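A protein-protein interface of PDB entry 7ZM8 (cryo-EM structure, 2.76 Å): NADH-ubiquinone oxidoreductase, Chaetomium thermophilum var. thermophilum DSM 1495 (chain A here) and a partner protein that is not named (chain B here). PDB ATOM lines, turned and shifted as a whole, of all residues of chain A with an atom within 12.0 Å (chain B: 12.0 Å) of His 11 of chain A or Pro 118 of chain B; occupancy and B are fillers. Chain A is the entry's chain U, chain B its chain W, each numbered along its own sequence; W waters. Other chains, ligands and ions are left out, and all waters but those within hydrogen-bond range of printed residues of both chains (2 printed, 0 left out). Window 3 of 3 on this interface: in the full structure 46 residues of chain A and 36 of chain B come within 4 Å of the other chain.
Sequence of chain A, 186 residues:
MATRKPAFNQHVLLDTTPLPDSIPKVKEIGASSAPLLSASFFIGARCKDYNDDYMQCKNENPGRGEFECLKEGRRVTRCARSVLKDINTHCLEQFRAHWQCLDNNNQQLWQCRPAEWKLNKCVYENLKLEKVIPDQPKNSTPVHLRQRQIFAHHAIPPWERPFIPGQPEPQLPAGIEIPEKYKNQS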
ATOM      1  N   MET A   1      -2.708 -24.710 -15.182  1.00  0.00           N
ATOM      2  CA  MET A   1      -3.993 -24.186 -14.658  1.00  0.00           C
ATOM      3  C   MET A   1      -4.308 -24.892 -13.361  1.00  0.00           C
ATOM      4  O   MET A   1      -3.552 -25.799 -13.020  1.00  0.00           O
ATOM      5  CB  MET A   1      -5.136 -24.378 -15.646  1.00  0.00           C
ATOM      6  N   ALA A   2      -5.418 -24.558 -12.722  1.00  0.00           N
ATOM      7  CA  ALA A   2      -5.686 -25.088 -11.371  1.00  0.00           C
ATOM      8  C   ALA A   2      -5.694 -26.606 -11.341  1.00  0.00           C
ATOM      9  O   ALA A   2      -6.183 -27.211 -12.282  1.00  0.00           O
ATOM     10  CB  ALA A   2      -6.951 -24.506 -10.839  1.00  0.00           C
ATOM     11  N   ARG A   4      -7.329 -28.454  -9.295  1.00  0.00           N
ATOM     12  CA  ARG A   4      -8.632 -28.967  -8.820  1.00  0.00           C
ATOM     13  C   ARG A   4      -9.239 -29.868  -9.882  1.00  0.00           C
ATOM     14  O   ARG A   4      -9.144 -29.522 -11.049  1.00  0.00           O
ATOM     15  CB  ARG A   4      -9.587 -27.789  -8.629  1.00  0.00           C
ATOM     16  CG  ARG A   4     -11.018 -28.190  -8.319  1.00  0.00           C
ATOM     17  CD  ARG A   4     -11.959 -27.009  -8.255  1.00  0.00           C
ATOM     18  NE  ARG A   4     -11.751 -26.032  -9.310  1.00  0.00           N
ATOM     19  CZ  ARG A   4     -12.400 -26.010 -10.465  1.00  0.00           C
ATOM     20  NH1 ARG A   4     -12.137 -25.065 -11.349  1.00  0.00           N
ATOM     21  NH2 ARG A   4     -13.307 -26.931 -10.733  1.00  0.00           N
ATOM     22  N   LYS A   5      -9.813 -31.003  -9.482  1.00  0.00           N
ATOM     23  CA  LYS A   5     -10.532 -31.865 -10.439  1.00  0.00           C
ATOM     24  C   LYS A   5     -11.775 -31.090 -10.890  1.00  0.00           C
ATOM     25  O   LYS A   5     -12.455 -30.518 -10.022  1.00  0.00           O
ATOM     26  CB  LYS A   5     -10.907 -33.137  -9.695  1.00  0.00           C
ATOM     27  CG  LYS A   5      -9.738 -33.957  -9.167  1.00  0.00           C
ATOM     28  CD  LYS A   5     -10.143 -34.915  -8.068  1.00  0.00           C
ATOM     29  CE  LYS A   5      -9.296 -36.167  -8.032  1.00  0.00           C
ATOM     30  NZ  LYS A   5      -9.590 -37.052  -9.184  1.00  0.00           N
ATOM     31  N   PRO A   6     -12.122 -31.043 -12.193  1.00  0.00           N
ATOM     32  CA  PRO A   6     -13.326 -30.344 -12.608  1.00  0.00           C
ATOM     33  C   PRO A   6     -14.654 -31.105 -12.425  1.00  0.00           C
ATOM     34  O   PRO A   6     -14.669 -32.298 -12.609  1.00  0.00           O
ATOM     35  CB  PRO A   6     -12.969 -30.033 -14.060  1.00  0.00           C
ATOM     36  CG  PRO A   6     -12.154 -31.214 -14.515  1.00  0.00           C
ATOM     37  CD  PRO A   6     -11.358 -31.617 -13.296  1.00  0.00           C
ATOM     38  N   ALA A   7     -15.742 -30.392 -12.106  1.00  0.00           N
ATOM     39  CA  ALA A   7     -17.025 -31.041 -11.902  1.00  0.00           C
ATOM     40  C   ALA A   7     -18.034 -30.780 -13.007  1.00  0.00           C
ATOM     41  O   ALA A   7     -18.860 -31.656 -13.276  1.00  0.00           O
ATOM     42  CB  ALA A   7     -17.639 -30.599 -10.563  1.00  0.00           C
ATOM     43  N   PHE A   8     -17.964 -29.608 -13.634  1.00  0.00           N
ATOM     44  CA  PHE A   8     -18.951 -29.221 -14.671  1.00  0.00           C
ATOM     45  C   PHE A   8     -18.209 -28.731 -15.918  1.00  0.00           C
ATOM     46  O   PHE A   8     -18.592 -27.693 -16.468  1.00  0.00           O
ATOM     47  CB  PHE A   8     -19.903 -28.161 -14.113  1.00  0.00           C
ATOM     48  CG  PHE A   8     -20.484 -28.485 -12.763  1.00  0.00           C
ATOM     49  CD1 PHE A   8     -21.454 -29.461 -12.623  1.00  0.00           C
ATOM     50  CD2 PHE A   8     -20.057 -27.813 -11.631  1.00  0.00           C
ATOM     51  CE1 PHE A   8     -21.977 -29.763 -11.378  1.00  0.00           C
ATOM     52  CE2 PHE A   8     -20.580 -28.116 -10.386  1.00  0.00           C
ATOM     53  CZ  PHE A   8     -21.537 -29.093 -10.264  1.00  0.00           C
ATOM     54  N   ASN A   9     -17.169 -29.447 -16.338  1.00  0.00           N
ATOM     55  CA  ASN A   9     -16.365 -29.049 -17.524  1.00  0.00           C
ATOM     56  C   ASN A   9     -17.092 -29.482 -18.798  1.00  0.00           C
ATOM     57  O   ASN A   9     -17.365 -30.666 -18.923  1.00  0.00           O
ATOM     58  CB  ASN A   9     -14.968 -29.674 -17.478  1.00  0.00           C
ATOM     59  CG  ASN A   9     -14.952 -31.127 -17.047  1.00  0.00           C
ATOM     60  OD1 ASN A   9     -15.585 -31.508 -16.066  1.00  0.00           O
ATOM     61  ND2 ASN A   9     -14.202 -31.950 -17.759  1.00  0.00           N
ATOM     62  N   GLN A  10     -17.380 -28.551 -19.709  1.00  0.00           N
ATOM     63  CA  GLN A  10     -18.008 -28.931 -21.000  1.00  0.00           C
ATOM     64  C   GLN A  10     -17.136 -28.485 -22.172  1.00  0.00           C
ATOM     65  O   GLN A  10     -17.391 -28.951 -23.287  1.00  0.00           O
ATOM     66  CB  GLN A  10     -19.398 -28.295 -21.111  1.00  0.00           C
ATOM     67  CG  GLN A  10     -20.351 -28.696 -19.994  1.00  0.00           C
ATOM     68  CD  GLN A  10     -20.816 -30.125 -20.121  1.00  0.00           C
ATOM     69  OE1 GLN A  10     -20.816 -30.709 -21.201  1.00  0.00           O
ATOM     70  NE2 GLN A  10     -21.231 -30.699 -19.006  1.00  0.00           N
ATOM     71  N   HIS A  11     -16.140 -27.634 -21.922  1.00  0.00           N
ATOM     72  CA  HIS A  11     -15.330 -27.060 -23.029  1.00  0.00           C
ATOM     73  C   HIS A  11     -13.833 -27.154 -22.734  1.00  0.00           C
ATOM     74  O   HIS A  11     -13.464 -27.153 -21.556  1.00  0.00           O
ATOM     75  CB  HIS A  11     -15.760 -25.610 -23.306  1.00  0.00           C
ATOM     76  CG  HIS A  11     -17.174 -25.470 -23.754  1.00  0.00           C
ATOM     77  ND1 HIS A  11     -17.595 -25.885 -24.999  1.00  0.00           N
ATOM     78  CD2 HIS A  11     -18.259 -24.961 -23.136  1.00  0.00           C
ATOM     79  CE1 HIS A  11     -18.882 -25.642 -25.128  1.00  0.00           C
ATOM     80  NE2 HIS A  11     -19.312 -25.076 -23.999  1.00  0.00           N
ATOM     81  N   VAL A  12     -13.010 -27.217 -23.783  1.00  0.00           N
ATOM     82  CA  VAL A  12     -11.529 -27.295 -23.635  1.00  0.00           C
ATOM     83  C   VAL A  12     -10.930 -26.039 -24.266  1.00  0.00           C
ATOM     84  O   VAL A  12     -11.393 -25.657 -25.350  1.00  0.00           O
ATOM     85  CB  VAL A  12     -10.972 -28.576 -24.285  1.00  0.00           C
ATOM     86  CG1 VAL A  12      -9.518 -28.432 -24.697  1.00  0.00           C
ATOM     87  CG2 VAL A  12     -11.162 -29.792 -23.394  1.00  0.00           C
ATOM     88  N   LEU A  13      -9.982 -25.397 -23.583  1.00  0.00           N
ATOM     89  CA  LEU A  13      -9.290 -24.227 -24.179  1.00  0.00           C
ATOM     90  C   LEU A  13      -7.891 -24.643 -24.628  1.00  0.00           C
ATOM     91  O   LEU A  13      -7.095 -25.034 -23.768  1.00  0.00           O
ATOM     92  CB  LEU A  13      -9.236 -23.073 -23.176  1.00  0.00           C
ATOM     93  CG  LEU A  13      -8.640 -21.769 -23.700  1.00  0.00           C
ATOM     94  CD1 LEU A  13      -9.428 -21.248 -24.888  1.00  0.00           C
ATOM     95  CD2 LEU A  13      -8.589 -20.725 -22.598  1.00  0.00           C
ATOM     96  N   LEU A  14      -7.630 -24.586 -25.932  1.00  0.00           N
ATOM     97  CA  LEU A  14      -6.283 -24.890 -26.457  1.00  0.00           C
ATOM     98  C   LEU A  14      -5.577 -23.575 -26.760  1.00  0.00           C
ATOM     99  O   LEU A  14      -6.257 -22.540 -26.820  1.00  0.00           O
ATOM    100  CB  LEU A  14      -6.392 -25.756 -27.714  1.00  0.00           C
ATOM    101  CG  LEU A  14      -6.937 -27.167 -27.503  1.00  0.00           C
ATOM    102  CD1 LEU A  14      -6.919 -27.948 -28.805  1.00  0.00           C
ATOM    103  CD2 LEU A  14      -6.138 -27.901 -26.442  1.00  0.00           C
ATOM    104  N   ASP A  15      -4.260 -23.622 -26.913  1.00  0.00           N
ATOM    105  CA  ASP A  15      -3.440 -22.455 -27.205  1.00  0.00           C
ATOM    106  C   ASP A  15      -2.385 -22.860 -28.220  1.00  0.00           C
ATOM    107  O   ASP A  15      -1.476 -23.629 -27.894  1.00  0.00           O
ATOM    108  CB  ASP A  15      -2.793 -21.915 -25.928  1.00  0.00           C
ATOM    109  CG  ASP A  15      -2.443 -20.445 -26.022  1.00  0.00           C
ATOM    110  OD1 ASP A  15      -2.691 -19.827 -27.076  1.00  0.00           O
ATOM    111  OD2 ASP A  15      -1.920 -19.904 -25.028  1.00  0.00           O
ATOM    112  N   ARG B  82       1.916 -21.441 -22.160  1.00  0.00           N
ATOM    113  CA  ARG B  82       0.666 -20.648 -22.108  1.00  0.00           C
ATOM    114  C   ARG B  82       0.861 -19.361 -21.331  1.00  0.00           C
ATOM    115  O   ARG B  82       0.183 -18.391 -21.646  1.00  0.00           O
ATOM    116  CB  ARG B  82      -0.439 -21.563 -21.572  1.00  0.00           C
ATOM    117  CG  ARG B  82      -0.615 -22.809 -22.427  1.00  0.00           C
ATOM    118  CD  ARG B  82      -1.888 -23.602 -22.236  1.00  0.00           C
ATOM    119  NE  ARG B  82      -3.086 -22.795 -22.366  1.00  0.00           N
ATOM    120  CZ  ARG B  82      -4.272 -23.278 -22.696  1.00  0.00           C
ATOM    121  NH1 ARG B  82      -5.313 -22.473 -22.789  1.00  0.00           N
ATOM    122  NH2 ARG B  82      -4.411 -24.563 -22.951  1.00  0.00           N
ATOM    123  N   THR B 110      -6.358 -19.534 -12.441  1.00  0.00           N
ATOM    124  CA  THR B 110      -7.705 -19.903 -11.929  1.00  0.00           C
ATOM    125  C   THR B 110      -8.706 -19.613 -13.036  1.00  0.00           C
ATOM    126  O   THR B 110      -9.573 -20.450 -13.264  1.00  0.00           O
ATOM    127  CB  THR B 110      -8.048 -19.206 -10.607  1.00  0.00           C
ATOM    128  OG1 THR B 110      -6.981 -19.506  -9.716  1.00  0.00           O
ATOM    129  CG2 THR B 110      -9.372 -19.638 -10.018  1.00  0.00           C
ATOM    130  N   PHE B 111      -8.576 -18.443 -13.656  1.00  0.00           N
ATOM    131  CA  PHE B 111      -9.481 -18.024 -14.744  1.00  0.00           C
ATOM    132  C   PHE B 111      -8.627 -17.859 -15.993  1.00  0.00           C
ATOM    133  O   PHE B 111      -7.417 -17.711 -15.867  1.00  0.00           O
ATOM    134  CB  PHE B 111     -10.127 -16.702 -14.364  1.00  0.00           C
ATOM    135  CG  PHE B 111     -10.812 -16.650 -13.027  1.00  0.00           C
ATOM    136  CD1 PHE B 111     -12.078 -17.178 -12.865  1.00  0.00           C
ATOM    137  CD2 PHE B 111     -10.213 -16.021 -11.951  1.00  0.00           C
ATOM    138  CE1 PHE B 111     -12.722 -17.092 -11.645  1.00  0.00           C
ATOM    139  CE2 PHE B 111     -10.851 -15.956 -10.726  1.00  0.00           C
ATOM    140  CZ  PHE B 111     -12.104 -16.493 -10.575  1.00  0.00           C
ATOM    141  N   ALA B 112      -9.244 -17.924 -17.163  1.00  0.00           N
ATOM    142  CA  ALA B 112      -8.520 -17.732 -18.439  1.00  0.00           C
ATOM    143  C   ALA B 112      -9.361 -16.878 -19.376  1.00  0.00           C
ATOM    144  O   ALA B 112     -10.583 -16.823 -19.189  1.00  0.00           O
ATOM    145  CB  ALA B 112      -8.285 -19.066 -19.077  1.00  0.00           C
ATOM    146  N   VAL B 113      -8.740 -16.240 -20.360  1.00  0.00           N
ATOM    147  CA  VAL B 113      -9.549 -15.496 -21.370  1.00  0.00           C
ATOM    148  C   VAL B 113     -10.033 -16.551 -22.345  1.00  0.00           C
ATOM    149  O   VAL B 113      -9.255 -17.443 -22.676  1.00  0.00           O
ATOM    150  CB  VAL B 113      -8.780 -14.355 -22.058  1.00  0.00           C
ATOM    151  CG1 VAL B 113      -9.515 -13.791 -23.252  1.00  0.00           C
ATOM    152  CG2 VAL B 113      -8.399 -13.265 -21.076  1.00  0.00           C
ATOM    153  N   THR B 114     -11.294 -16.466 -22.741  1.00  0.00           N
ATOM    154  CA  THR B 114     -11.873 -17.515 -23.599  1.00  0.00           C
ATOM    155  C   THR B 114     -12.426 -16.864 -24.855  1.00  0.00           C
ATOM    156  O   THR B 114     -12.818 -15.694 -24.791  1.00  0.00           O
ATOM    157  CB  THR B 114     -12.942 -18.314 -22.843  1.00  0.00           C
ATOM    158  OG1 THR B 114     -13.814 -17.388 -22.202  1.00  0.00           O
ATOM    159  CG2 THR B 114     -12.368 -19.280 -21.831  1.00  0.00           C
ATOM    160  N   PRO B 115     -12.444 -17.541 -26.033  1.00  0.00           N
ATOM    161  CA  PRO B 115     -13.100 -16.971 -27.194  1.00  0.00           C
ATOM    162  C   PRO B 115     -14.590 -16.803 -26.885  1.00  0.00           C
ATOM    163  O   PRO B 115     -15.108 -17.537 -26.077  1.00  0.00           O
ATOM    164  CB  PRO B 115     -12.909 -18.026 -28.282  1.00  0.00           C
ATOM    165  CG  PRO B 115     -11.655 -18.742 -27.877  1.00  0.00           C
ATOM    166  CD  PRO B 115     -11.788 -18.823 -26.376  1.00  0.00           C
ATOM    167  N   SER B 116     -15.246 -15.860 -27.555  1.00  0.00           N
ATOM    168  CA  SER B 116     -16.683 -15.585 -27.308  1.00  0.00           C
ATOM    169  C   SER B 116     -17.537 -16.807 -27.647  1.00  0.00           C
ATOM    170  O   SER B 116     -18.527 -17.031 -26.939  1.00  0.00           O
ATOM    171  CB  SER B 116     -17.114 -14.369 -28.069  1.00  0.00           C
ATOM    172  OG  SER B 116     -16.578 -14.386 -29.383  1.00  0.00           O
ATOM    173  N   LYS B 117     -17.190 -17.542 -28.707  1.00  0.00           N
ATOM    174  CA  LYS B 117     -18.010 -18.706 -29.134  1.00  0.00           C
ATOM    175  C   LYS B 117     -17.171 -19.980 -29.336  1.00  0.00           C
ATOM    176  O   LYS B 117     -16.016 -19.847 -29.765  1.00  0.00           O
ATOM    177  CB  LYS B 117     -18.735 -18.407 -30.450  1.00  0.00           C
ATOM    178  CG  LYS B 117     -19.731 -17.256 -30.411  1.00  0.00           C
ATOM    179  CD  LYS B 117     -20.903 -17.502 -29.484  1.00  0.00           C
ATOM    180  CE  LYS B 117     -21.813 -18.615 -29.958  1.00  0.00           C
ATOM    181  NZ  LYS B 117     -22.441 -18.290 -31.261  1.00  0.00           N
ATOM    182  N   PRO B 118     -17.685 -21.211 -29.070  1.00  0.00           N
ATOM    183  CA  PRO B 118     -16.941 -22.425 -29.380  1.00  0.00           C
ATOM    184  C   PRO B 118     -16.864 -22.741 -30.880  1.00  0.00           C
ATOM    185  O   PRO B 118     -17.615 -22.156 -31.637  1.00  0.00           O
ATOM    186  CB  PRO B 118     -17.797 -23.509 -28.737  1.00  0.00           C
ATOM    187  CG  PRO B 118     -18.644 -22.787 -27.725  1.00  0.00           C
ATOM    188  CD  PRO B 118     -18.961 -21.484 -28.417  1.00  0.00           C
ATOM    189  N   ALA B 119     -15.981 -23.663 -31.273  1.00  0.00           N
ATOM    190  CA  ALA B 119     -15.854 -24.076 -32.694  1.00  0.00           C
ATOM    191  C   ALA B 119     -17.194 -24.606 -33.215  1.00  0.00           C
ATOM    192  O   ALA B 119     -17.836 -25.380 -32.482  1.00  0.00           O
ATOM    193  CB  ALA B 119     -14.762 -25.102 -32.828  1.00  0.00           C
ATOM    194  N   GLN B 120     -17.585 -24.228 -34.437  1.00  0.00           N
ATOM    195  CA  GLN B 120     -18.915 -24.607 -34.999  1.00  0.00           C
ATOM    196  C   GLN B 120     -19.290 -26.070 -34.749  1.00  0.00           C
ATOM    197  O   GLN B 120     -20.440 -26.291 -34.323  1.00  0.00           O
ATOM    198  CB  GLN B 120     -18.976 -24.275 -36.490  1.00  0.00           C
ATOM    199  CG  GLN B 120     -19.353 -22.829 -36.783  1.00  0.00           C
ATOM    200  CD  GLN B 120     -18.249 -21.850 -36.465  1.00  0.00           C
ATOM    201  OE1 GLN B 120     -18.482 -20.791 -35.884  1.00  0.00           O
ATOM    202  NE2 GLN B 120     -17.030 -22.200 -36.838  1.00  0.00           N
ATOM    203  N   GLU B 121     -18.399 -27.019 -35.056  1.00  0.00           N
ATOM    204  CA  GLU B 121     -18.683 -28.445 -34.893  1.00  0.00           C
ATOM    205  C   GLU B 121     -19.825 -28.902 -35.797  1.00  0.00           C
ATOM    206  O   GLU B 121     -20.012 -28.373 -36.892  1.00  0.00           O
ATOM    207  CB  GLU B 121     -19.012 -28.767 -33.433  1.00  0.00           C
HETATM  208  O   HOH W   1      -9.931 -23.100 -11.320  1.00  0.00           O
HETATM  209  O   HOH W   2      -2.731 -19.023 -22.740  1.00  0.00           O
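NH2 of Arg 82 of chain B is in hydrogen-bond range of O of Leu 13 of chain A (2.8 Å).
Pro 118 of chain B touches His 11 of chain A (CG to CE1, 3.9 Å). Ala 112 of chain B touches Leu 13 of chain A (CB to CD2, 3.9 Å). Val 113 of chain B touches Leu 13 of chain A (O to CD2, 3.3 Å). CD1 of Leu 13 of chain A touches CD of Pro 115 of chain B, 3.7 Å away. NH2 of Arg 82 of chain B touches CA of Leu 14 of chain A, at 3.99 Å. CB of Asp 15 of chain A touches NE of Arg 82 of chain B, 3.7 Å away.
Pro 6 of chain A touches none of the printed residues of chain B. No residue of chain B comes within 4 Å of Asn 9 of chain A. No residue of chain B comes within 4 Å of Gln 10 of chain A. Of chain B, only Pro 118 (3.9 Å) comes within 4 Å of His 11 of chain A. Val 12 of chain A touches none of the printed residues of chain B. Printed residues of chain B within 4 Å of Leu 13 of chain A: Arg 82 (2.8 Å), Ala 112 (3.9 Å), Val 113 (3.3 Å) and Pro 115 (3.7 Å). Printed residues of chain A within 4 Å of Val 113 of chain B: Leu 13 (3.3 Å). Pro 115 of chain B touches just one residue of chain A: Leu 13 (3.7 Å). No residue of chain A comes within 4 Å of Ser 116 of chain B. No residue of chain A comes within 4 Å of Ala 119 of chain B. The nearest printed residue of chain B that does not touch Leu 13 of chain A is Thr 114 of chain B (4.1 Å).
Hydrophobic or aromatic side chains of chain B within 4 Å of the printed part of chain A: Ala 112, Pro 115 and Pro 118. Hydrophobic or aromatic side chains of chain A within 4 Å of the printed part of chain B: His 11 and Leu 13. Among the printed residues, 7 pairs touch across the chains.
Water W2 bridges OD2 of Asp 15 of chain A (2.6 Å) and O of Arg 82 of chain B (3.2 Å). Water W1 lies within hydrogen-bond range of the guanidinium group of Arg 4 of chain A (3.0 Å) and the backbone carbonyl oxygen of Thr 110 of chain B (3.3 Å).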
